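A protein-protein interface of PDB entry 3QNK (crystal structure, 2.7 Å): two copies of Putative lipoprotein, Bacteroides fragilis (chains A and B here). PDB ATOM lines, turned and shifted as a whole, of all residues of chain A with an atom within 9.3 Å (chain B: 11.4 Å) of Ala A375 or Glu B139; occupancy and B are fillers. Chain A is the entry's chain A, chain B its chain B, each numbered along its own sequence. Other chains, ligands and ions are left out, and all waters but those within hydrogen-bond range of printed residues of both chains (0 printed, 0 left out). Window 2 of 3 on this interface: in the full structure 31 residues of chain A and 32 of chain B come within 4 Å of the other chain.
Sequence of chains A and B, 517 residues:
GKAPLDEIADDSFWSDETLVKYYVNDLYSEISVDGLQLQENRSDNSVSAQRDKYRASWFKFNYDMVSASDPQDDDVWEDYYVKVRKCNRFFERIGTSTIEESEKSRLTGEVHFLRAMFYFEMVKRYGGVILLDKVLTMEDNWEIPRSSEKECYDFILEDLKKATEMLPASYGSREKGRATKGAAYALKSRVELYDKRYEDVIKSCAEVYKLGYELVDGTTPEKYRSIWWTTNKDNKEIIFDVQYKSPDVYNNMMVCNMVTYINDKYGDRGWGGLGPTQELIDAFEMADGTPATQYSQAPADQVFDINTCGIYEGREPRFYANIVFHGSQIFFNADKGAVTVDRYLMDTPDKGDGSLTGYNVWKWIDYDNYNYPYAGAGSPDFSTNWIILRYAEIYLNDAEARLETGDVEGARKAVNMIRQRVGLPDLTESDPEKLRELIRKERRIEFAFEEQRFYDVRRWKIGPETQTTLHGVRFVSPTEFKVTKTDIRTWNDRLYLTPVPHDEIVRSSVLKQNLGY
The guanidinium group of Arg A269 lies within hydrogen-bond range of the backbone carbonyl oxygen of Met B138, at 3.0 Å.
NH2 of Arg A269 is in hydrogen-bond range of O of Asp B140.
The backbone carbonyl oxygen (O) of Gly A376 lies close to the backbone carbonyl oxygen (O) of Glu B139 (3.0 Å).
The side-chain hydroxyl (OH) of Tyr A372 is in hydrogen-bond range of the backbone NH (N) of Arg A269 (3.0 Å).
The guanidinium group (NH1) of Arg A269 sits at hydrogen-bond distance from the backbone carbonyl oxygen (O) of Pro A373 (2.8 Å).
N of Thr B137 lies within hydrogen-bond range of OD2 of Asp B140 (2.7 Å).
O of Thr B137 is in hydrogen-bond range of NE1 of Trp B142 (2.8 Å).
Among the printed residues, pairs that only touch across the chains: Pro A247 with Arg B85 (3.5 Å), Pro A247 with Trp B142 (3.3 Å), Val A249 with Met B138 (3.5 Å), Val A249 with Trp B142 (3.4 Å), Arg A269 with Trp B142 (3.9 Å), Ala A375 with Met B138 (3.7 Å), Ala A375 with Glu B139 (3.4 Å) and Ala A375 with Asp B140 (3.9 Å).
Glu B139 touches just these residues of chain A: Ala A375 and Gly A376.
Gly A376 touches one residue of chain B.
No residue of chain B comes within 4 Å of Ala A377.
Printed residues of chain B within 4 Å of Arg A269: Met B138 (3.0 Å), Asp B140 (2.9 Å) and Trp B142 (3.9 Å).
Of the printed residues of chain A, Trp B142 touches Pro A247 (3.3 Å), Val A249 (3.4 Å) and Arg A269 (3.9 Å).
Of the printed residues of chain A, Met B138 touches Val A249, Arg A269 and Ala A375.
Printed residues of chain B within 4 Å of Val A249: Met B138 (3.5 Å) and Trp B142 (3.4 Å).
Printed residues of chain A within 4 Å of Arg B85: Pro A247.
Asn B141 touches none of the printed residues of chain A.
The nearest residue of chain B that does not touch Ala A375 is Asn B141 (4.7 Å).
Of the 14 printed residues of chain A, 5 touch a printed residue of chain B.
Hydrophobic or aromatic side chains of chain A within 4 Å of the printed part of chain B: Pro A247, Val A249 and Ala A375.
Among the printed residues, no Asp or Glu carboxylate lies within 4 Å of a Lys or Arg side-chain nitrogen of the other chain.
No position is printed for both chains.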
ATOM      1  N   PRO A 247     -15.888   0.461 -12.113  1.00  0.00           N
ATOM      2  CA  PRO A 247     -15.630  -0.057 -10.750  1.00  0.00           C
ATOM      3  C   PRO A 247     -14.764  -1.342 -10.765  1.00  0.00           C
ATOM      4  O   PRO A 247     -13.692  -1.371 -10.135  1.00  0.00           O
ATOM      5  CB  PRO A 247     -17.039  -0.314 -10.171  1.00  0.00           C
ATOM      6  CG  PRO A 247     -18.010   0.336 -11.108  1.00  0.00           C
ATOM      7  CD  PRO A 247     -17.338   0.471 -12.439  1.00  0.00           C
ATOM      8  N   VAL A 249     -12.456  -4.613 -12.298  1.00  0.00           N
ATOM      9  CA  VAL A 249     -11.293  -5.002 -13.104  1.00  0.00           C
ATOM     10  C   VAL A 249     -11.750  -5.746 -14.373  1.00  0.00           C
ATOM     11  O   VAL A 249     -11.052  -5.731 -15.393  1.00  0.00           O
ATOM     12  CB  VAL A 249     -10.301  -5.863 -12.241  1.00  0.00           C
ATOM     13  CG1 VAL A 249     -10.715  -7.333 -12.148  1.00  0.00           C
ATOM     14  CG2 VAL A 249      -8.869  -5.751 -12.745  1.00  0.00           C
ATOM     15  N   VAL A 255      -7.666  -2.191 -18.452  1.00  0.00           N
ATOM     16  CA  VAL A 255      -7.214  -3.528 -18.087  1.00  0.00           C
ATOM     17  C   VAL A 255      -7.731  -4.549 -19.095  1.00  0.00           C
ATOM     18  O   VAL A 255      -6.958  -5.408 -19.535  1.00  0.00           O
ATOM     19  CB  VAL A 255      -7.610  -3.869 -16.629  1.00  0.00           C
ATOM     20  CG1 VAL A 255      -7.231  -5.301 -16.256  1.00  0.00           C
ATOM     21  CG2 VAL A 255      -6.973  -2.872 -15.648  1.00  0.00           C
ATOM     22  N   TYR A 266       6.323  -6.578 -15.467  1.00  0.00           N
ATOM     23  CA  TYR A 266       5.146  -6.090 -14.746  1.00  0.00           C
ATOM     24  C   TYR A 266       4.220  -7.207 -14.231  1.00  0.00           C
ATOM     25  O   TYR A 266       4.448  -7.675 -13.118  1.00  0.00           O
ATOM     26  CB  TYR A 266       4.404  -5.073 -15.598  1.00  0.00           C
ATOM     27  CG  TYR A 266       5.205  -3.805 -15.737  1.00  0.00           C
ATOM     28  CD1 TYR A 266       5.459  -2.995 -14.629  1.00  0.00           C
ATOM     29  CD2 TYR A 266       5.790  -3.453 -16.953  1.00  0.00           C
ATOM     30  CE1 TYR A 266       6.206  -1.830 -14.741  1.00  0.00           C
ATOM     31  CE2 TYR A 266       6.565  -2.295 -17.072  1.00  0.00           C
ATOM     32  CZ  TYR A 266       6.770  -1.487 -15.958  1.00  0.00           C
ATOM     33  OH  TYR A 266       7.503  -0.327 -16.042  1.00  0.00           O
ATOM     34  N   GLY A 267       3.197  -7.593 -14.987  1.00  0.00           N
ATOM     35  CA  GLY A 267       2.271  -8.636 -14.562  1.00  0.00           C
ATOM     36  C   GLY A 267       1.346  -9.117 -15.656  1.00  0.00           C
ATOM     37  O   GLY A 267       1.461  -8.675 -16.806  1.00  0.00           O
ATOM     38  N   ASP A 268       0.381  -9.974 -15.288  1.00  0.00           N
ATOM     39  CA  ASP A 268      -0.603 -10.529 -16.220  1.00  0.00           C
ATOM     40  C   ASP A 268      -2.040 -10.091 -15.892  1.00  0.00           C
ATOM     41  O   ASP A 268      -3.024 -10.787 -16.233  1.00  0.00           O
ATOM     42  CB  ASP A 268      -0.506 -12.061 -16.278  1.00  0.00           C
ATOM     43  CG  ASP A 268      -0.499 -12.796 -14.945  1.00  0.00           C
ATOM     44  OD1 ASP A 268      -0.958 -12.207 -13.923  1.00  0.00           O
ATOM     45  OD2 ASP A 268      -0.054 -13.961 -14.923  1.00  0.00           O
ATOM     46  N   ARG A 269      -2.152  -8.888 -15.323  1.00  0.00           N
ATOM     47  CA  ARG A 269      -3.418  -8.280 -14.927  1.00  0.00           C
ATOM     48  C   ARG A 269      -4.340  -8.007 -16.154  1.00  0.00           C
ATOM     49  O   ARG A 269      -5.557  -8.116 -16.004  1.00  0.00           O
ATOM     50  CB  ARG A 269      -3.164  -7.000 -14.114  1.00  0.00           C
ATOM     51  CG  ARG A 269      -4.342  -6.539 -13.301  1.00  0.00           C
ATOM     52  CD  ARG A 269      -3.993  -6.499 -11.855  1.00  0.00           C
ATOM     53  NE  ARG A 269      -5.192  -6.515 -11.016  1.00  0.00           N
ATOM     54  CZ  ARG A 269      -5.684  -5.453 -10.400  1.00  0.00           C
ATOM     55  NH1 ARG A 269      -5.082  -4.279 -10.507  1.00  0.00           N
ATOM     56  NH2 ARG A 269      -6.765  -5.563  -9.642  1.00  0.00           N
ATOM     57  N   TYR A 372       1.943   0.853 -14.206  1.00  0.00           N
ATOM     58  CA  TYR A 372       1.266  -0.439 -14.331  1.00  0.00           C
ATOM     59  C   TYR A 372       0.195  -0.600 -13.231  1.00  0.00           C
ATOM     60  O   TYR A 372       0.479  -0.323 -12.063  1.00  0.00           O
ATOM     61  CB  TYR A 372       2.261  -1.606 -14.279  1.00  0.00           C
ATOM     62  CG  TYR A 372       1.623  -2.942 -14.600  1.00  0.00           C
ATOM     63  CD1 TYR A 372       1.363  -3.311 -15.917  1.00  0.00           C
ATOM     64  CD2 TYR A 372       1.251  -3.827 -13.586  1.00  0.00           C
ATOM     65  CE1 TYR A 372       0.752  -4.528 -16.220  1.00  0.00           C
ATOM     66  CE2 TYR A 372       0.648  -5.053 -13.879  1.00  0.00           C
ATOM     67  CZ  TYR A 372       0.402  -5.399 -15.199  1.00  0.00           C
ATOM     68  OH  TYR A 372      -0.205  -6.585 -15.526  1.00  0.00           O
ATOM     69  N   PRO A 373      -1.035  -1.065 -13.583  1.00  0.00           N
ATOM     70  CA  PRO A 373      -2.082  -1.202 -12.553  1.00  0.00           C
ATOM     71  C   PRO A 373      -1.886  -2.414 -11.628  1.00  0.00           C
ATOM     72  O   PRO A 373      -2.654  -3.389 -11.698  1.00  0.00           O
ATOM     73  CB  PRO A 373      -3.364  -1.325 -13.379  1.00  0.00           C
ATOM     74  CG  PRO A 373      -2.926  -1.922 -14.651  1.00  0.00           C
ATOM     75  CD  PRO A 373      -1.546  -1.416 -14.925  1.00  0.00           C
ATOM     76  N   TYR A 374      -0.900  -2.332 -10.713  1.00  0.00           N
ATOM     77  CA  TYR A 374      -0.669  -3.430  -9.765  1.00  0.00           C
ATOM     78  C   TYR A 374      -1.801  -3.528  -8.768  1.00  0.00           C
ATOM     79  O   TYR A 374      -2.309  -2.498  -8.317  1.00  0.00           O
ATOM     80  CB  TYR A 374       0.632  -3.276  -8.952  1.00  0.00           C
ATOM     81  CG  TYR A 374       1.935  -3.012  -9.678  1.00  0.00           C
ATOM     82  CD1 TYR A 374       2.750  -4.065 -10.092  1.00  0.00           C
ATOM     83  CD2 TYR A 374       2.446  -1.719  -9.781  1.00  0.00           C
ATOM     84  CE1 TYR A 374       4.004  -3.832 -10.656  1.00  0.00           C
ATOM     85  CE2 TYR A 374       3.692  -1.472 -10.355  1.00  0.00           C
ATOM     86  CZ  TYR A 374       4.477  -2.533 -10.778  1.00  0.00           C
ATOM     87  OH  TYR A 374       5.712  -2.289 -11.336  1.00  0.00           O
ATOM     88  N   ALA A 375      -2.142  -4.759  -8.357  1.00  0.00           N
ATOM     89  CA  ALA A 375      -3.142  -4.962  -7.314  1.00  0.00           C
ATOM     90  C   ALA A 375      -2.449  -4.790  -5.977  1.00  0.00           C
ATOM     91  O   ALA A 375      -2.168  -5.769  -5.302  1.00  0.00           O
ATOM     92  CB  ALA A 375      -3.773  -6.346  -7.437  1.00  0.00           C
ATOM     93  N   GLY A 376      -2.081  -3.559  -5.657  1.00  0.00           N
ATOM     94  CA  GLY A 376      -1.384  -3.245  -4.421  1.00  0.00           C
ATOM     95  C   GLY A 376      -2.168  -2.230  -3.632  1.00  0.00           C
ATOM     96  O   GLY A 376      -3.248  -2.538  -3.127  1.00  0.00           O
ATOM     97  N   ALA A 377      -1.644  -1.004  -3.560  1.00  0.00           N
ATOM     98  CA  ALA A 377      -2.252   0.124  -2.858  1.00  0.00           C
ATOM     99  C   ALA A 377      -1.927   1.409  -3.625  1.00  0.00           C
ATOM    100  O   ALA A 377      -1.883   1.394  -4.864  1.00  0.00           O
ATOM    101  CB  ALA A 377      -1.745   0.185  -1.422  1.00  0.00           C
ATOM    102  N   PHE A 382      -7.635   3.860 -12.589  1.00  0.00           N
ATOM    103  CA  PHE A 382      -7.132   3.771 -13.951  1.00  0.00           C
ATOM    104  C   PHE A 382      -8.230   4.038 -14.960  1.00  0.00           C
ATOM    105  O   PHE A 382      -8.797   3.134 -15.576  1.00  0.00           O
ATOM    106  CB  PHE A 382      -6.464   2.431 -14.178  1.00  0.00           C
ATOM    107  CG  PHE A 382      -5.122   2.431 -13.508  1.00  0.00           C
ATOM    108  CD1 PHE A 382      -4.024   3.008 -14.126  1.00  0.00           C
ATOM    109  CD2 PHE A 382      -4.971   1.931 -12.220  1.00  0.00           C
ATOM    110  CE1 PHE A 382      -2.783   3.046 -13.492  1.00  0.00           C
ATOM    111  CE2 PHE A 382      -3.728   1.976 -11.580  1.00  0.00           C
ATOM    112  CZ  PHE A 382      -2.639   2.524 -12.228  1.00  0.00           C
ATOM    113  N   ARG B  85     -22.939  -3.369  -3.353  1.00  0.00           N
ATOM    114  CA  ARG B  85     -21.883  -2.359  -3.514  1.00  0.00           C
ATOM    115  C   ARG B  85     -22.316  -1.019  -2.880  1.00  0.00           C
ATOM    116  O   ARG B  85     -21.525  -0.415  -2.149  1.00  0.00           O
ATOM    117  CB  ARG B  85     -21.504  -2.180  -4.985  1.00  0.00           C
ATOM    118  CG  ARG B  85     -20.302  -1.254  -5.206  1.00  0.00           C
ATOM    119  CD  ARG B  85     -19.972  -1.062  -6.677  1.00  0.00           C
ATOM    120  NE  ARG B  85     -18.706  -0.353  -6.844  1.00  0.00           N
ATOM    121  CZ  ARG B  85     -18.603   0.940  -7.126  1.00  0.00           C
ATOM    122  NH1 ARG B  85     -19.691   1.678  -7.285  1.00  0.00           N
ATOM    123  NH2 ARG B  85     -17.409   1.509  -7.244  1.00  0.00           N
ATOM    124  N   GLU B  92     -18.468   2.291   4.402  1.00  0.00           N
ATOM    125  CA  GLU B  92     -17.146   2.895   4.250  1.00  0.00           C
ATOM    126  C   GLU B  92     -17.131   4.382   4.589  1.00  0.00           C
ATOM    127  O   GLU B  92     -16.173   4.857   5.200  1.00  0.00           O
ATOM    128  CB  GLU B  92     -16.619   2.736   2.805  1.00  0.00           C
ATOM    129  CG  GLU B  92     -16.130   1.340   2.441  1.00  0.00           C
ATOM    130  CD  GLU B  92     -15.621   1.132   1.024  1.00  0.00           C
ATOM    131  OE1 GLU B  92     -15.837   2.013   0.158  1.00  0.00           O
ATOM    132  OE2 GLU B  92     -15.007   0.067   0.782  1.00  0.00           O
ATOM    133  N   LYS B 134     -16.630  -4.672   1.592  1.00  0.00           N
ATOM    134  CA  LYS B 134     -16.010  -3.428   1.131  1.00  0.00           C
ATOM    135  C   LYS B 134     -16.276  -3.264  -0.363  1.00  0.00           C
ATOM    136  O   LYS B 134     -16.631  -4.240  -1.045  1.00  0.00           O
ATOM    137  CB  LYS B 134     -14.490  -3.386   1.444  1.00  0.00           C
ATOM    138  CG  LYS B 134     -13.628  -4.516   0.836  1.00  0.00           C
ATOM    139  CD  LYS B 134     -12.668  -4.031  -0.273  1.00  0.00           C
ATOM    140  CE  LYS B 134     -11.364  -3.372   0.160  1.00  0.00           C
ATOM    141  N   VAL B 135     -16.134  -2.023  -0.855  1.00  0.00           N
ATOM    142  CA  VAL B 135     -16.259  -1.698  -2.275  1.00  0.00           C
ATOM    143  C   VAL B 135     -14.915  -2.017  -2.904  1.00  0.00           C
ATOM    144  O   VAL B 135     -13.888  -1.471  -2.494  1.00  0.00           O
ATOM    145  CB  VAL B 135     -16.714  -0.237  -2.533  1.00  0.00           C
ATOM    146  CG1 VAL B 135     -16.685   0.081  -4.022  1.00  0.00           C
ATOM    147  CG2 VAL B 135     -18.102   0.029  -1.944  1.00  0.00           C
ATOM    148  N   LEU B 136     -14.900  -2.964  -3.833  1.00  0.00           N
ATOM    149  CA  LEU B 136     -13.656  -3.378  -4.467  1.00  0.00           C
ATOM    150  C   LEU B 136     -13.165  -2.288  -5.372  1.00  0.00           C
ATOM    151  O   LEU B 136     -13.960  -1.600  -6.016  1.00  0.00           O
ATOM    152  CB  LEU B 136     -13.789  -4.708  -5.219  1.00  0.00           C
ATOM    153  CG  LEU B 136     -14.085  -5.966  -4.435  1.00  0.00           C
ATOM    154  CD1 LEU B 136     -14.470  -7.073  -5.360  1.00  0.00           C
ATOM    155  CD2 LEU B 136     -12.901  -6.397  -3.633  1.00  0.00           C
ATOM    156  N   THR B 137     -11.848  -2.112  -5.362  1.00  0.00           N
ATOM    157  CA  THR B 137     -11.078  -1.120  -6.112  1.00  0.00           C
ATOM    158  C   THR B 137      -9.993  -1.843  -6.960  1.00  0.00           C
ATOM    159  O   THR B 137      -9.895  -3.064  -6.898  1.00  0.00           O
ATOM    160  CB  THR B 137     -10.494  -0.088  -5.111  1.00  0.00           C
ATOM    161  OG1 THR B 137      -9.529   0.711  -5.781  1.00  0.00           O
ATOM    162  CG2 THR B 137      -9.793  -0.722  -3.938  1.00  0.00           C
ATOM    163  N   MET B 138      -9.195  -1.095  -7.742  1.00  0.00           N
ATOM    164  CA  MET B 138      -8.061  -1.628  -8.492  1.00  0.00           C
ATOM    165  C   MET B 138      -7.040  -2.234  -7.555  1.00  0.00           C
ATOM    166  O   MET B 138      -6.370  -3.178  -7.938  1.00  0.00           O
ATOM    167  CB  MET B 138      -7.372  -0.530  -9.305  1.00  0.00           C
ATOM    168  CG  MET B 138      -7.946  -0.333 -10.679  1.00  0.00           C
ATOM    169  SD  MET B 138      -7.825  -1.923 -11.831  1.00  0.00           S
ATOM    170  CE  MET B 138      -9.764  -2.005 -12.282  1.00  0.00           C
ATOM    171  N   GLU B 139      -6.927  -1.693  -6.326  1.00  0.00           N
ATOM    172  CA  GLU B 139      -5.989  -2.147  -5.300  1.00  0.00           C
ATOM    173  C   GLU B 139      -6.287  -3.587  -4.853  1.00  0.00           C
ATOM    174  O   GLU B 139      -5.400  -4.282  -4.358  1.00  0.00           O
ATOM    175  CB  GLU B 139      -6.040  -1.196  -4.089  1.00  0.00           C
ATOM    176  N   ASP B 140      -7.519  -4.031  -5.064  1.00  0.00           N
ATOM    177  CA  ASP B 140      -7.983  -5.353  -4.653  1.00  0.00           C
ATOM    178  C   ASP B 140      -7.775  -6.439  -5.716  1.00  0.00           C
ATOM    179  O   ASP B 140      -7.671  -6.163  -6.915  1.00  0.00           O
ATOM    180  CB  ASP B 140      -9.484  -5.282  -4.292  1.00  0.00           C
ATOM    181  CG  ASP B 140      -9.812  -4.310  -3.180  1.00  0.00           C
ATOM    182  OD1 ASP B 140      -9.131  -4.347  -2.142  1.00  0.00           O
ATOM    183  OD2 ASP B 140     -10.789  -3.562  -3.318  1.00  0.00           O
ATOM    184  N   ASN B 141      -7.726  -7.686  -5.246  1.00  0.00           N
ATOM    185  CA  ASN B 141      -7.667  -8.849  -6.112  1.00  0.00           C
ATOM    186  C   ASN B 141      -9.099  -9.255  -6.364  1.00  0.00           C
ATOM    187  O   ASN B 141      -9.855  -9.462  -5.410  1.00  0.00           O
ATOM    188  CB  ASN B 141      -6.855  -9.960  -5.478  1.00  0.00           C
ATOM    189  CG  ASN B 141      -7.080 -11.304  -6.096  1.00  0.00           C
ATOM    190  OD1 ASN B 141      -7.123 -11.457  -7.326  1.00  0.00           O
ATOM    191  ND2 ASN B 141      -7.270 -12.297  -5.234  1.00  0.00           N
ATOM    192  N   TRP B 142      -9.494  -9.334  -7.622  1.00  0.00           N
ATOM    193  CA  TRP B 142     -10.886  -9.622  -7.923  1.00  0.00           C
ATOM    194  C   TRP B 142     -11.176 -11.093  -8.121  1.00  0.00           C
ATOM    195  O   TRP B 142     -12.350 -11.455  -8.205  1.00  0.00           O
ATOM    196  CB  TRP B 142     -11.324  -8.823  -9.131  1.00  0.00           C
ATOM    197  CG  TRP B 142     -11.417  -7.351  -8.843  1.00  0.00           C
ATOM    198  CD1 TRP B 142     -10.379  -6.482  -8.634  1.00  0.00           C
ATOM    199  CD2 TRP B 142     -12.620  -6.569  -8.778  1.00  0.00           C
ATOM    200  NE1 TRP B 142     -10.864  -5.214  -8.410  1.00  0.00           N
ATOM    201  CE2 TRP B 142     -12.234  -5.232  -8.521  1.00  0.00           C
ATOM    202  CE3 TRP B 142     -13.990  -6.865  -8.958  1.00  0.00           C
ATOM    203  CZ2 TRP B 142     -13.167  -4.190  -8.447  1.00  0.00           C
ATOM    204  CZ3 TRP B 142     -14.924  -5.856  -8.781  1.00  0.00           C
ATOM    205  CH2 TRP B 142     -14.517  -4.536  -8.531  1.00  0.00           C
ATOM    206  N   GLU B 143     -10.146 -11.953  -8.142  1.00  0.00           N
ATOM    207  CA  GLU B 143     -10.399 -13.378  -8.236  1.00  0.00           C
ATOM    208  C   GLU B 143     -10.687 -13.856  -6.809  1.00  0.00           C
ATOM    209  O   GLU B 143      -9.794 -14.218  -6.041  1.00  0.00           O
ATOM    210  CB  GLU B 143      -9.276 -14.141  -8.955  1.00  0.00           C
ATOM    211  CG  GLU B 143      -9.199 -13.835 -10.450  1.00  0.00           C
ATOM    212  CD  GLU B 143      -9.233 -14.998 -11.430  1.00  0.00           C
ATOM    213  OE1 GLU B 143      -8.801 -16.113 -11.055  1.00  0.00           O
ATOM    214  OE2 GLU B 143      -9.632 -14.774 -12.599  1.00  0.00           O
ATOM    215  N   ILE B 144     -11.951 -13.716  -6.433  1.00  0.00           N
ATOM    216  CA  ILE B 144     -12.456 -14.076  -5.127  1.00  0.00           C
ATOM    217  C   ILE B 144     -13.392 -15.272  -5.283  1.00  0.00           C
ATOM    218  O   ILE B 144     -14.362 -15.189  -6.043  1.00  0.00           O
ATOM    219  CB  ILE B 144     -13.163 -12.887  -4.422  1.00  0.00           C
ATOM    220  CG1 ILE B 144     -12.278 -11.647  -4.380  1.00  0.00           C
ATOM    221  CG2 ILE B 144     -13.625 -13.280  -3.020  1.00  0.00           C
ATOM    222  CD1 ILE B 144     -13.019 -10.380  -4.410  1.00  0.00           C
